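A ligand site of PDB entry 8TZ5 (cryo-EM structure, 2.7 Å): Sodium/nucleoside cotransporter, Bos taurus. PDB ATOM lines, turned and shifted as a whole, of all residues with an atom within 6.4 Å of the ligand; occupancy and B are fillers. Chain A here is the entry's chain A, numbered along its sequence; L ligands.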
ATOM      1  N   VAL A 313       7.815  -9.998  23.355  1.00  0.00           N
ATOM      2  CA  VAL A 313       8.539 -11.264  23.348  1.00  0.00           C
ATOM      3  C   VAL A 313       8.238 -12.053  24.620  1.00  0.00           C
ATOM      4  O   VAL A 313       8.011 -13.262  24.573  1.00  0.00           O
ATOM      5  CB  VAL A 313      10.050 -11.014  23.191  1.00  0.00           C
ATOM      6  CG1 VAL A 313      10.811 -12.334  23.170  1.00  0.00           C
ATOM      7  CG2 VAL A 313      10.330 -10.220  21.931  1.00  0.00           C
ATOM      8  N   SER A 317       6.348 -15.641  24.594  1.00  0.00           N
ATOM      9  CA  SER A 317       7.005 -16.805  25.182  1.00  0.00           C
ATOM     10  C   SER A 317       6.116 -17.457  26.241  1.00  0.00           C
ATOM     11  O   SER A 317       5.987 -18.685  26.286  1.00  0.00           O
ATOM     12  CB  SER A 317       8.341 -16.406  25.795  1.00  0.00           C
ATOM     13  OG  SER A 317       9.187 -15.809  24.823  1.00  0.00           O
ATOM     14  N   ILE A 360       8.793 -22.930  16.939  1.00  0.00           N
ATOM     15  CA  ILE A 360       9.769 -22.979  18.015  1.00  0.00           C
ATOM     16  C   ILE A 360      11.136 -22.603  17.460  1.00  0.00           C
ATOM     17  O   ILE A 360      11.417 -22.760  16.272  1.00  0.00           O
ATOM     18  CB  ILE A 360       9.817 -24.387  18.666  1.00  0.00           C
ATOM     19  CG1 ILE A 360       8.436 -24.757  19.222  1.00  0.00           C
ATOM     20  CG2 ILE A 360      10.850 -24.416  19.779  1.00  0.00           C
ATOM     21  CD1 ILE A 360       8.283 -26.224  19.548  1.00  0.00           C
ATOM     22  N   GLY A 361      11.989 -22.101  18.355  1.00  0.00           N
ATOM     23  CA  GLY A 361      13.327 -21.693  17.966  1.00  0.00           C
ATOM     24  C   GLY A 361      14.238 -22.874  17.679  1.00  0.00           C
ATOM     25  O   GLY A 361      13.905 -24.041  17.892  1.00  0.00           O
ATOM     26  N   GLN A 362      15.432 -22.544  17.190  1.00  0.00           N
ATOM     27  CA  GLN A 362      16.407 -23.561  16.826  1.00  0.00           C
ATOM     28  C   GLN A 362      17.056 -24.197  18.040  1.00  0.00           C
ATOM     29  O   GLN A 362      17.502 -25.347  17.968  1.00  0.00           O
ATOM     30  CB  GLN A 362      17.477 -22.959  15.916  1.00  0.00           C
ATOM     31  CG  GLN A 362      18.259 -21.818  16.533  1.00  0.00           C
ATOM     32  CD  GLN A 362      19.263 -21.218  15.584  1.00  0.00           C
ATOM     33  OE1 GLN A 362      19.582 -21.801  14.547  1.00  0.00           O
ATOM     34  NE2 GLN A 362      19.768 -20.035  15.924  1.00  0.00           N
ATOM     35  N   THR A 363      17.136 -23.470  19.152  1.00  0.00           N
ATOM     36  CA  THR A 363      17.764 -23.983  20.368  1.00  0.00           C
ATOM     37  C   THR A 363      16.807 -24.775  21.246  1.00  0.00           C
ATOM     38  O   THR A 363      17.258 -25.386  22.215  1.00  0.00           O
ATOM     39  CB  THR A 363      18.362 -22.823  21.171  1.00  0.00           C
ATOM     40  OG1 THR A 363      17.361 -21.831  21.410  1.00  0.00           O
ATOM     41  CG2 THR A 363      19.531 -22.195  20.415  1.00  0.00           C
ATOM     42  N   GLU A 364      15.514 -24.766  20.944  1.00  0.00           N
ATOM     43  CA  GLU A 364      14.521 -25.506  21.719  1.00  0.00           C
ATOM     44  C   GLU A 364      13.789 -26.566  20.913  1.00  0.00           C
ATOM     45  O   GLU A 364      13.185 -27.457  21.521  1.00  0.00           O
ATOM     46  CB  GLU A 364      13.494 -24.548  22.331  1.00  0.00           C
ATOM     47  CG  GLU A 364      14.072 -23.538  23.306  1.00  0.00           C
ATOM     48  CD  GLU A 364      14.814 -22.409  22.627  1.00  0.00           C
ATOM     49  OE1 GLU A 364      14.595 -22.178  21.425  1.00  0.00           O
ATOM     50  OE2 GLU A 364      15.640 -21.752  23.306  1.00  0.00           O
ATOM     51  N   ALA A 393      11.069 -18.001  15.315  1.00  0.00           N
ATOM     52  CA  ALA A 393      10.295 -18.449  16.454  1.00  0.00           C
ATOM     53  C   ALA A 393       9.115 -17.501  16.664  1.00  0.00           C
ATOM     54  O   ALA A 393       9.190 -16.321  16.327  1.00  0.00           O
ATOM     55  CB  ALA A 393      11.143 -18.510  17.726  1.00  0.00           C
ATOM     56  N   GLY A 394       8.037 -18.045  17.223  1.00  0.00           N
ATOM     57  CA  GLY A 394       6.857 -17.235  17.460  1.00  0.00           C
ATOM     58  C   GLY A 394       7.097 -16.135  18.473  1.00  0.00           C
ATOM     59  O   GLY A 394       6.378 -15.128  18.487  1.00  0.00           O
ATOM     60  N   SER A 395       8.098 -16.304  19.335  1.00  0.00           N
ATOM     61  CA  SER A 395       8.382 -15.294  20.354  1.00  0.00           C
ATOM     62  C   SER A 395       8.785 -13.961  19.735  1.00  0.00           C
ATOM     63  O   SER A 395       8.411 -12.892  20.237  1.00  0.00           O
ATOM     64  CB  SER A 395       9.466 -15.798  21.293  1.00  0.00           C
ATOM     65  OG  SER A 395      10.650 -16.119  20.584  1.00  0.00           O
ATOM     66  N   VAL A 396       9.539 -13.998  18.627  1.00  0.00           N
ATOM     67  CA  VAL A 396      10.034 -12.784  17.992  1.00  0.00           C
ATOM     68  C   VAL A 396       9.173 -12.359  16.812  1.00  0.00           C
ATOM     69  O   VAL A 396       9.503 -11.361  16.141  1.00  0.00           O
ATOM     70  CB  VAL A 396      11.500 -12.949  17.546  1.00  0.00           C
ATOM     71  CG1 VAL A 396      12.393 -13.159  18.756  1.00  0.00           C
ATOM     72  CG2 VAL A 396      11.637 -14.100  16.562  1.00  0.00           C
ATOM     73  N   TYR A 400       8.827  -8.247  14.979  1.00  0.00           N
ATOM     74  CA  TYR A 400       8.880  -7.939  13.558  1.00  0.00           C
ATOM     75  C   TYR A 400       7.572  -7.336  13.075  1.00  0.00           C
ATOM     76  O   TYR A 400       7.589  -6.435  12.224  1.00  0.00           O
ATOM     77  CB  TYR A 400       9.208  -9.205  12.760  1.00  0.00           C
ATOM     78  CG  TYR A 400      10.457  -9.916  13.209  1.00  0.00           C
ATOM     79  CD1 TYR A 400      11.526  -9.210  13.756  1.00  0.00           C
ATOM     80  CD2 TYR A 400      10.586 -11.292  13.089  1.00  0.00           C
ATOM     81  CE1 TYR A 400      12.673  -9.850  14.163  1.00  0.00           C
ATOM     82  CE2 TYR A 400      11.727 -11.944  13.500  1.00  0.00           C
ATOM     83  CZ  TYR A 400      12.764 -11.220  14.038  1.00  0.00           C
ATOM     84  OH  TYR A 400      13.911 -11.860  14.444  1.00  0.00           O
ATOM     85  N   LEU A 467      16.738 -14.193  26.854  1.00  0.00           N
ATOM     86  CA  LEU A 467      16.480 -13.921  25.447  1.00  0.00           C
ATOM     87  C   LEU A 467      16.502 -12.423  25.159  1.00  0.00           C
ATOM     88  O   LEU A 467      17.230 -11.954  24.275  1.00  0.00           O
ATOM     89  CB  LEU A 467      15.136 -14.532  25.052  1.00  0.00           C
ATOM     90  CG  LEU A 467      14.667 -14.340  23.611  1.00  0.00           C
ATOM     91  CD1 LEU A 467      15.624 -15.002  22.647  1.00  0.00           C
ATOM     92  CD2 LEU A 467      13.254 -14.878  23.450  1.00  0.00           C
ATOM     93  N   ILE A 471      19.272 -10.188  23.161  1.00  0.00           N
ATOM     94  CA  ILE A 471      18.853  -9.417  21.995  1.00  0.00           C
ATOM     95  C   ILE A 471      19.326  -7.972  22.122  1.00  0.00           C
ATOM     96  O   ILE A 471      19.951  -7.421  21.203  1.00  0.00           O
ATOM     97  CB  ILE A 471      17.320  -9.488  21.833  1.00  0.00           C
ATOM     98  CG1 ILE A 471      16.894 -10.896  21.413  1.00  0.00           C
ATOM     99  CG2 ILE A 471      16.842  -8.458  20.817  1.00  0.00           C
ATOM    100  CD1 ILE A 471      15.417 -11.155  21.567  1.00  0.00           C
ATOM    101  N   ASN A 474      23.298  -7.676  22.047  1.00  0.00           N
ATOM    102  CA  ASN A 474      23.807  -7.946  20.711  1.00  0.00           C
ATOM    103  C   ASN A 474      23.472  -6.815  19.746  1.00  0.00           C
ATOM    104  O   ASN A 474      24.301  -6.439  18.911  1.00  0.00           O
ATOM    105  CB  ASN A 474      23.244  -9.265  20.186  1.00  0.00           C
ATOM    106  CG  ASN A 474      23.809 -10.474  20.898  1.00  0.00           C
ATOM    107  OD1 ASN A 474      24.422 -10.343  21.961  1.00  0.00           O
ATOM    108  ND2 ASN A 474      23.620 -11.654  20.319  1.00  0.00           N
ATOM    109  N   PHE A 538      25.007  -9.523  10.780  1.00  0.00           N
ATOM    110  CA  PHE A 538      24.644  -9.230  12.157  1.00  0.00           C
ATOM    111  C   PHE A 538      23.434 -10.063  12.629  1.00  0.00           C
ATOM    112  O   PHE A 538      23.590 -10.898  13.514  1.00  0.00           O
ATOM    113  CB  PHE A 538      24.345  -7.739  12.319  1.00  0.00           C
ATOM    114  CG  PHE A 538      25.452  -6.853  11.819  1.00  0.00           C
ATOM    115  CD1 PHE A 538      26.582  -6.649  12.587  1.00  0.00           C
ATOM    116  CD2 PHE A 538      25.364  -6.235  10.592  1.00  0.00           C
ATOM    117  CE1 PHE A 538      27.609  -5.842  12.135  1.00  0.00           C
ATOM    118  CE2 PHE A 538      26.377  -5.424  10.130  1.00  0.00           C
ATOM    119  CZ  PHE A 538      27.501  -5.232  10.903  1.00  0.00           C
ATOM    120  N   ASN A 539      22.271  -9.874  12.033  1.00  0.00           N
ATOM    121  CA  ASN A 539      21.089 -10.665  12.384  1.00  0.00           C
ATOM    122  C   ASN A 539      19.893 -10.230  11.547  1.00  0.00           C
ATOM    123  O   ASN A 539      20.004  -9.332  10.712  1.00  0.00           O
ATOM    124  CB  ASN A 539      20.777 -10.546  13.883  1.00  0.00           C
ATOM    125  CG  ASN A 539      20.756  -9.119  14.370  1.00  0.00           C
ATOM    126  OD1 ASN A 539      20.740  -8.178  13.567  1.00  0.00           O
ATOM    127  ND2 ASN A 539      20.755  -8.945  15.681  1.00  0.00           N
ATOM    128  N   GLU A 540      18.739 -10.861  11.765  1.00  0.00           N
ATOM    129  CA  GLU A 540      17.519 -10.510  11.050  1.00  0.00           C
ATOM    130  C   GLU A 540      16.762  -9.360  11.696  1.00  0.00           C
ATOM    131  O   GLU A 540      15.821  -8.840  11.094  1.00  0.00           O
ATOM    132  CB  GLU A 540      16.591 -11.723  10.922  1.00  0.00           C
ATOM    133  CG  GLU A 540      15.891 -12.164  12.215  1.00  0.00           C
ATOM    134  CD  GLU A 540      16.823 -12.769  13.230  1.00  0.00           C
ATOM    135  OE1 GLU A 540      17.983 -13.085  12.872  1.00  0.00           O
ATOM    136  OE2 GLU A 540      16.411 -12.943  14.397  1.00  0.00           O
ATOM    137  N   PHE A 541      17.152  -8.938  12.909  1.00  0.00           N
ATOM    138  CA  PHE A 541      16.510  -7.789  13.533  1.00  0.00           C
ATOM    139  C   PHE A 541      16.854  -6.502  12.801  1.00  0.00           C
ATOM    140  O   PHE A 541      15.972  -5.690  12.498  1.00  0.00           O
ATOM    141  CB  PHE A 541      16.941  -7.695  14.997  1.00  0.00           C
ATOM    142  CG  PHE A 541      15.980  -8.340  15.962  1.00  0.00           C
ATOM    143  CD1 PHE A 541      14.937  -7.610  16.512  1.00  0.00           C
ATOM    144  CD2 PHE A 541      16.117  -9.671  16.323  1.00  0.00           C
ATOM    145  CE1 PHE A 541      14.052  -8.197  17.394  1.00  0.00           C
ATOM    146  CE2 PHE A 541      15.232 -10.259  17.205  1.00  0.00           C
ATOM    147  CZ  PHE A 541      14.206  -9.524  17.741  1.00  0.00           C
ATOM    148  N   GLY A 583      14.685 -15.916   8.832  1.00  0.00           N
ATOM    149  CA  GLY A 583      15.562 -16.990   9.260  1.00  0.00           C
ATOM    150  C   GLY A 583      16.581 -16.569  10.294  1.00  0.00           C
ATOM    151  O   GLY A 583      16.978 -15.398  10.353  1.00  0.00           O
ATOM    152  N   PHE A 584      17.013 -17.524  11.119  1.00  0.00           N
ATOM    153  CA  PHE A 584      18.048 -17.300  12.121  1.00  0.00           C
ATOM    154  C   PHE A 584      19.440 -17.651  11.613  1.00  0.00           C
ATOM    155  O   PHE A 584      20.306 -18.053  12.406  1.00  0.00           O
ATOM    156  CB  PHE A 584      17.734 -18.083  13.394  1.00  0.00           C
ATOM    157  CG  PHE A 584      16.536 -17.580  14.161  1.00  0.00           C
ATOM    158  CD1 PHE A 584      15.955 -16.357  13.880  1.00  0.00           C
ATOM    159  CD2 PHE A 584      15.993 -18.341  15.186  1.00  0.00           C
ATOM    160  CE1 PHE A 584      14.869 -15.909  14.589  1.00  0.00           C
ATOM    161  CE2 PHE A 584      14.908 -17.890  15.904  1.00  0.00           C
ATOM    162  CZ  PHE A 584      14.345 -16.675  15.601  1.00  0.00           C
ATOM    163  N   ALA A 585      19.677 -17.519  10.312  1.00  0.00           N
ATOM    164  CA  ALA A 585      20.946 -17.905   9.710  1.00  0.00           C
ATOM    165  C   ALA A 585      21.911 -16.723   9.776  1.00  0.00           C
ATOM    166  O   ALA A 585      21.771 -15.755   9.031  1.00  0.00           O
ATOM    167  CB  ALA A 585      20.750 -18.371   8.273  1.00  0.00           C
ATOM    168  N   ASN A 586      22.884 -16.821  10.667  1.00  0.00           N
ATOM    169  CA  ASN A 586      23.969 -15.867  10.721  1.00  0.00           C
ATOM    170  C   ASN A 586      25.170 -16.566  11.324  1.00  0.00           C
ATOM    171  O   ASN A 586      25.045 -17.621  11.952  1.00  0.00           O
ATOM    172  CB  ASN A 586      23.585 -14.603  11.509  1.00  0.00           C
ATOM    173  CG  ASN A 586      23.252 -14.896  12.967  1.00  0.00           C
ATOM    174  OD1 ASN A 586      24.144 -15.142  13.776  1.00  0.00           O
ATOM    175  ND2 ASN A 586      21.966 -14.866  13.301  1.00  0.00           N
ATOM    176  N   GLY A 588      26.993 -15.717  13.809  1.00  0.00           N
ATOM    177  CA  GLY A 588      26.912 -15.766  15.260  1.00  0.00           C
ATOM    178  C   GLY A 588      26.049 -16.916  15.755  1.00  0.00           C
ATOM    179  O   GLY A 588      26.348 -17.510  16.790  1.00  0.00           O
ATOM    180  N   SER A 589      24.982 -17.242  15.019  1.00  0.00           N
ATOM    181  CA  SER A 589      24.123 -18.354  15.419  1.00  0.00           C
ATOM    182  C   SER A 589      24.884 -19.669  15.366  1.00  0.00           C
ATOM    183  O   SER A 589      24.525 -20.631  16.055  1.00  0.00           O
ATOM    184  CB  SER A 589      22.893 -18.405  14.522  1.00  0.00           C
ATOM    185  OG  SER A 589      22.221 -17.158  14.494  1.00  0.00           O
ATOM    186  N   ILE A 592      26.571 -20.746  18.805  1.00  0.00           N
ATOM    187  CA  ILE A 592      25.633 -21.019  19.885  1.00  0.00           C
ATOM    188  C   ILE A 592      24.821 -22.277  19.569  1.00  0.00           C
ATOM    189  O   ILE A 592      24.542 -23.091  20.454  1.00  0.00           O
ATOM    190  CB  ILE A 592      24.723 -19.798  20.150  1.00  0.00           C
ATOM    191  CG1 ILE A 592      23.849 -19.495  18.932  1.00  0.00           C
ATOM    192  CG2 ILE A 592      25.576 -18.601  20.464  1.00  0.00           C
ATOM    193  CD1 ILE A 592      22.489 -20.147  18.972  1.00  0.00           C
ATOM    194  N   VAL A 593      24.462 -22.458  18.294  1.00  0.00           N
ATOM    195  CA  VAL A 593      23.777 -23.683  17.883  1.00  0.00           C
ATOM    196  C   VAL A 593      24.665 -24.888  18.186  1.00  0.00           C
ATOM    197  O   VAL A 593      24.206 -25.895  18.737  1.00  0.00           O
ATOM    198  CB  VAL A 593      23.429 -23.609  16.378  1.00  0.00           C
ATOM    199  CG1 VAL A 593      23.094 -24.987  15.817  1.00  0.00           C
ATOM    200  CG2 VAL A 593      22.292 -22.652  16.167  1.00  0.00           C
HETATM  201  C1  LIG L   1      18.713 -15.641  18.252  1.00  0.00           C
HETATM  202  C2  LIG L   1      17.583 -17.773  19.034  1.00  0.00           C
HETATM  203  C3  LIG L   1      15.141 -17.738  19.706  1.00  0.00           C
HETATM  204  C4  LIG L   1      15.097 -16.279  19.409  1.00  0.00           C
HETATM  205  C5  LIG L   1      16.315 -15.578  18.918  1.00  0.00           C
HETATM  206  C6  LIG L   1      18.956 -13.716  17.131  1.00  0.00           C
HETATM  207  C7  LIG L   1      18.138 -12.600  16.849  1.00  0.00           C
HETATM  208  C8  LIG L   1      18.701 -14.825  16.050  1.00  0.00           C
HETATM  209  C9  LIG L   1      18.885 -15.916  16.642  1.00  0.00           C
HETATM  210  N1  LIG L   1      16.375 -18.471  19.522  1.00  0.00           N
HETATM  211  N2  LIG L   1      13.967 -18.393  20.175  1.00  0.00           N
HETATM  212  N3  LIG L   1      17.538 -16.317  18.727  1.00  0.00           N
HETATM  213  O1  LIG L   1      18.582 -18.377  18.879  1.00  0.00           O
HETATM  214  O2  LIG L   1      12.790 -17.670  20.352  1.00  0.00           O
HETATM  215  O3  LIG L   1      18.573 -14.367  18.434  1.00  0.00           O
HETATM  216  O4  LIG L   1      16.810 -12.990  16.980  1.00  0.00           O
HETATM  217  O5  LIG L   1      19.668 -14.684  14.907  1.00  0.00           O
HETATM  218  O6  LIG L   1      20.253 -16.415  16.369  1.00  0.00           O
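OE2 of Glu 540 sits at hydrogen-bond distance from O4 of the ligand.
OG of Ser 395 is in hydrogen-bond range of O2 of the ligand (2.7 Å).
The side-chain amide nitrogen (ND2) of Asn 586 sits at hydrogen-bond distance from an oxygen (O5) of the ligand (2.8 Å).
OG of Ser 589 sits at hydrogen-bond distance from O6 of the ligand, 2.8 Å away.
OH of Tyr 400 sits at hydrogen-bond distance from OE2 of Glu 540, 2.7 Å away.
The side-chain amide oxygen of Asn 586 lies within hydrogen-bond range of the backbone NH of Ser 589 (2.6 Å).
OD1 of Asn 586 lies within hydrogen-bond range of N of Gly 588 (2.9 Å).
The side-chain hydroxyl of Ser 589 lies within hydrogen-bond range of the backbone carbonyl oxygen of Phe 584 (3.0 Å).
The side-chain carboxylate (OE2) of Glu 364 sits at hydrogen-bond distance from the side-chain hydroxyl (OG1) of Thr 363, at 2.6 Å.
Gln 362 touches the ligand.
Thr 363 touches the ligand.
CB of Ala 393 touches O2 of the ligand, at 3.2 Å.
Leu 467 touches the ligand.
CE2 of Phe 541 touches O4 of the ligand, at 3.2 Å.
Phe 584 touches the ligand.
Within 4 Å of the ligand: Gln 362, Thr 363, Ala 393, Ser 395, Leu 467, Glu 540, Phe 541, Phe 584, Asn 586 and Ser 589.
The nearest printed residue that does not touch the ligand is Tyr 400 (4.01 Å).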
